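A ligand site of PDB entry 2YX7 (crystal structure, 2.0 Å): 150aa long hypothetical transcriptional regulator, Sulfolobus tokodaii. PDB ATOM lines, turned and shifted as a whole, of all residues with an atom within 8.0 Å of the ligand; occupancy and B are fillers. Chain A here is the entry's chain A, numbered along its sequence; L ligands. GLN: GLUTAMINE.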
ATOM      1  N   LEU A  20      29.838 -17.426 -23.883  1.00  0.00           N
ATOM      2  CA  LEU A  20      28.948 -17.828 -24.963  1.00  0.00           C
ATOM      3  C   LEU A  20      29.331 -19.205 -25.507  1.00  0.00           C
ATOM      4  O   LEU A  20      28.465 -20.061 -25.748  1.00  0.00           O
ATOM      5  CB  LEU A  20      29.020 -16.804 -26.097  1.00  0.00           C
ATOM      6  CG  LEU A  20      28.659 -15.367 -25.728  1.00  0.00           C
ATOM      7  CD1 LEU A  20      28.882 -14.468 -26.929  1.00  0.00           C
ATOM      8  CD2 LEU A  20      27.206 -15.293 -25.273  1.00  0.00           C
ATOM      9  N   ASP A  21      30.619 -19.405 -25.695  1.00  0.00           N
ATOM     10  CA  ASP A  21      31.136 -20.667 -26.215  1.00  0.00           C
ATOM     11  C   ASP A  21      30.663 -21.829 -25.369  1.00  0.00           C
ATOM     12  O   ASP A  21      30.296 -22.884 -25.885  1.00  0.00           O
ATOM     13  CB  ASP A  21      32.658 -20.626 -26.257  1.00  0.00           C
ATOM     14  CG  ASP A  21      33.172 -19.535 -27.166  1.00  0.00           C
ATOM     15  OD1 ASP A  21      33.012 -19.673 -28.403  1.00  0.00           O
ATOM     16  OD2 ASP A  21      33.729 -18.531 -26.653  1.00  0.00           O
ATOM     17  N   GLU A  22      30.672 -21.636 -24.050  1.00  0.00           N
ATOM     18  CA  GLU A  22      30.242 -22.685 -23.152  1.00  0.00           C
ATOM     19  C   GLU A  22      28.741 -22.917 -23.245  1.00  0.00           C
ATOM     20  O   GLU A  22      28.283 -24.058 -23.284  1.00  0.00           O
ATOM     21  CB  GLU A  22      30.643 -22.350 -21.716  1.00  0.00           C
ATOM     22  CG  GLU A  22      32.123 -22.502 -21.442  1.00  0.00           C
ATOM     23  CD  GLU A  22      32.472 -22.225 -19.992  1.00  0.00           C
ATOM     24  OE1 GLU A  22      32.374 -21.047 -19.566  1.00  0.00           O
ATOM     25  OE2 GLU A  22      32.849 -23.183 -19.285  1.00  0.00           O
ATOM     26  N   ILE A  23      27.984 -21.832 -23.308  1.00  0.00           N
ATOM     27  CA  ILE A  23      26.525 -21.946 -23.400  1.00  0.00           C
ATOM     28  C   ILE A  23      26.156 -22.553 -24.753  1.00  0.00           C
ATOM     29  O   ILE A  23      25.329 -23.471 -24.828  1.00  0.00           O
ATOM     30  CB  ILE A  23      25.843 -20.579 -23.262  1.00  0.00           C
ATOM     31  CG1 ILE A  23      26.236 -19.929 -21.932  1.00  0.00           C
ATOM     32  CG2 ILE A  23      24.330 -20.740 -23.331  1.00  0.00           C
ATOM     33  CD1 ILE A  23      25.701 -18.534 -21.733  1.00  0.00           C
ATOM     34  N   ALA A  24      26.772 -22.037 -25.805  1.00  0.00           N
ATOM     35  CA  ALA A  24      26.525 -22.523 -27.156  1.00  0.00           C
ATOM     36  C   ALA A  24      26.694 -24.044 -27.202  1.00  0.00           C
ATOM     37  O   ALA A  24      25.920 -24.757 -27.843  1.00  0.00           O
ATOM     38  CB  ALA A  24      27.483 -21.865 -28.122  1.00  0.00           C
ATOM     39  N   ARG A  25      27.717 -24.536 -26.499  1.00  0.00           N
ATOM     40  CA  ARG A  25      28.012 -25.970 -26.458  1.00  0.00           C
ATOM     41  C   ARG A  25      26.955 -26.752 -25.695  1.00  0.00           C
ATOM     42  O   ARG A  25      26.543 -27.846 -26.108  1.00  0.00           O
ATOM     43  CB  ARG A  25      29.379 -26.199 -25.809  1.00  0.00           C
ATOM     44  CG  ARG A  25      29.822 -27.669 -25.752  1.00  0.00           C
ATOM     45  CD  ARG A  25      31.249 -27.827 -25.208  1.00  0.00           C
ATOM     46  NE  ARG A  25      32.205 -26.974 -25.908  1.00  0.00           N
ATOM     47  CZ  ARG A  25      32.678 -25.825 -25.439  1.00  0.00           C
ATOM     48  NH1 ARG A  25      32.296 -25.390 -24.247  1.00  0.00           N
ATOM     49  NH2 ARG A  25      33.532 -25.102 -26.161  1.00  0.00           N
ATOM     50  N   ARG A  28      23.727 -26.533 -27.616  1.00  0.00           N
ATOM     51  CA  ARG A  28      24.019 -26.897 -28.996  1.00  0.00           C
ATOM     52  C   ARG A  28      23.392 -26.007 -30.064  1.00  0.00           C
ATOM     53  O   ARG A  28      22.479 -26.412 -30.763  1.00  0.00           O
ATOM     54  CB  ARG A  28      23.601 -28.346 -29.270  1.00  0.00           C
ATOM     55  CG  ARG A  28      24.293 -29.384 -28.400  1.00  0.00           C
ATOM     56  CD  ARG A  28      23.278 -30.057 -27.504  1.00  0.00           C
ATOM     57  NE  ARG A  28      22.234 -30.721 -28.276  1.00  0.00           N
ATOM     58  CZ  ARG A  28      21.096 -31.171 -27.762  1.00  0.00           C
ATOM     59  NH1 ARG A  28      20.852 -31.041 -26.473  1.00  0.00           N
ATOM     60  NH2 ARG A  28      20.204 -31.763 -28.556  1.00  0.00           N
ATOM     61  N   ILE A  29      23.898 -24.779 -30.171  1.00  0.00           N
ATOM     62  CA  ILE A  29      23.426 -23.841 -31.190  1.00  0.00           C
ATOM     63  C   ILE A  29      24.568 -22.911 -31.551  1.00  0.00           C
ATOM     64  O   ILE A  29      25.520 -22.760 -30.791  1.00  0.00           O
ATOM     65  CB  ILE A  29      22.233 -22.981 -30.691  1.00  0.00           C
ATOM     66  CG1 ILE A  29      22.721 -21.947 -29.680  1.00  0.00           C
ATOM     67  CG2 ILE A  29      21.163 -23.869 -30.081  1.00  0.00           C
ATOM     68  CD1 ILE A  29      21.725 -20.842 -29.418  1.00  0.00           C
ATOM     69  N   PRO A  30      24.497 -22.269 -32.728  1.00  0.00           N
ATOM     70  CA  PRO A  30      25.541 -21.350 -33.171  1.00  0.00           C
ATOM     71  C   PRO A  30      25.716 -20.196 -32.196  1.00  0.00           C
ATOM     72  O   PRO A  30      24.745 -19.580 -31.764  1.00  0.00           O
ATOM     73  CB  PRO A  30      25.035 -20.893 -34.533  1.00  0.00           C
ATOM     74  CG  PRO A  30      24.297 -22.095 -35.024  1.00  0.00           C
ATOM     75  CD  PRO A  30      23.523 -22.521 -33.802  1.00  0.00           C
ATOM     76  N   LYS A  31      26.974 -19.909 -31.852  1.00  0.00           N
ATOM     77  CA  LYS A  31      27.284 -18.838 -30.917  1.00  0.00           C
ATOM     78  C   LYS A  31      26.713 -17.503 -31.367  1.00  0.00           C
ATOM     79  O   LYS A  31      26.343 -16.669 -30.539  1.00  0.00           O
ATOM     80  CB  LYS A  31      28.792 -18.720 -30.745  1.00  0.00           C
ATOM     81  CG  LYS A  31      29.228 -17.683 -29.725  1.00  0.00           C
ATOM     82  CD  LYS A  31      30.718 -17.772 -29.436  1.00  0.00           C
ATOM     83  CE  LYS A  31      31.545 -17.554 -30.690  1.00  0.00           C
ATOM     84  NZ  LYS A  31      33.010 -17.743 -30.464  1.00  0.00           N
ATOM     85  N   SER A  32      26.630 -17.289 -32.671  1.00  0.00           N
ATOM     86  CA  SER A  32      26.095 -16.046 -33.203  1.00  0.00           C
ATOM     87  C   SER A  32      24.585 -15.980 -32.989  1.00  0.00           C
ATOM     88  O   SER A  32      24.028 -14.893 -32.787  1.00  0.00           O
ATOM     89  CB  SER A  32      26.425 -15.937 -34.700  1.00  0.00           C
ATOM     90  OG  SER A  32      25.919 -17.060 -35.413  1.00  0.00           O
ATOM     91  N   THR A  33      23.926 -17.134 -33.051  1.00  0.00           N
ATOM     92  CA  THR A  33      22.478 -17.201 -32.845  1.00  0.00           C
ATOM     93  C   THR A  33      22.203 -16.888 -31.371  1.00  0.00           C
ATOM     94  O   THR A  33      21.343 -16.071 -31.043  1.00  0.00           O
ATOM     95  CB  THR A  33      21.952 -18.609 -33.155  1.00  0.00           C
ATOM     96  OG1 THR A  33      22.387 -18.986 -34.470  1.00  0.00           O
ATOM     97  CG2 THR A  33      20.428 -18.641 -33.114  1.00  0.00           C
ATOM     98  N   LEU A  34      22.958 -17.550 -30.499  1.00  0.00           N
ATOM     99  CA  LEU A  34      22.842 -17.338 -29.074  1.00  0.00           C
ATOM    100  C   LEU A  34      22.950 -15.853 -28.769  1.00  0.00           C
ATOM    101  O   LEU A  34      22.050 -15.245 -28.184  1.00  0.00           O
ATOM    102  CB  LEU A  34      23.967 -18.097 -28.347  1.00  0.00           C
ATOM    103  CG  LEU A  34      24.171 -17.799 -26.861  1.00  0.00           C
ATOM    104  CD1 LEU A  34      22.931 -18.191 -26.073  1.00  0.00           C
ATOM    105  CD2 LEU A  34      25.389 -18.552 -26.364  1.00  0.00           C
HETATM  106  N   GLN L   1      31.002 -20.185 -36.260  1.00  0.00           N
HETATM  107  CA  GLN L   1      29.584 -19.945 -35.838  1.00  0.00           C
HETATM  108  C   GLN L   1      29.396 -18.513 -35.364  1.00  0.00           C
HETATM  109  O   GLN L   1      30.197 -18.053 -34.511  1.00  0.00           O
HETATM  110  CB  GLN L   1      29.200 -20.907 -34.715  1.00  0.00           C
HETATM  111  CG  GLN L   1      30.024 -20.743 -33.447  1.00  0.00           C
HETATM  112  CD  GLN L   1      29.521 -21.600 -32.305  1.00  0.00           C
HETATM  113  OE1 GLN L   1      30.037 -21.528 -31.186  1.00  0.00           O
HETATM  114  NE2 GLN L   1      28.495 -22.402 -32.573  1.00  0.00           N
HETATM  115  OXT GLN L   1      28.457 -17.858 -35.858  1.00  0.00           O
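OG of Ser 32 lies within hydrogen-bond range of OXT of the ligand, 2.7 Å away. NE2 of the ligand lies within hydrogen-bond range of O of Ile 29 (3.5 Å).
The side-chain amino group of Lys 31 lies within salt-bridge range of the side-chain carboxylate of Asp 21, at 2.8 Å. The backbone NH (N) of Ile 29 lies within hydrogen-bond range of the backbone carbonyl oxygen (O) of Ala 24, 3.1 Å away.
The backbone NH (N) of Lys 31 sits close to a nitrogen (NE2) of the ligand, at 3.0 Å. Pro 30 touches the ligand (CA to NE2, 3.2 Å). Of the 13 residues printed, 4 come within 4 Å of the ligand. The nearest printed residue that does not touch the ligand is Ala 24 (4.003 Å).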
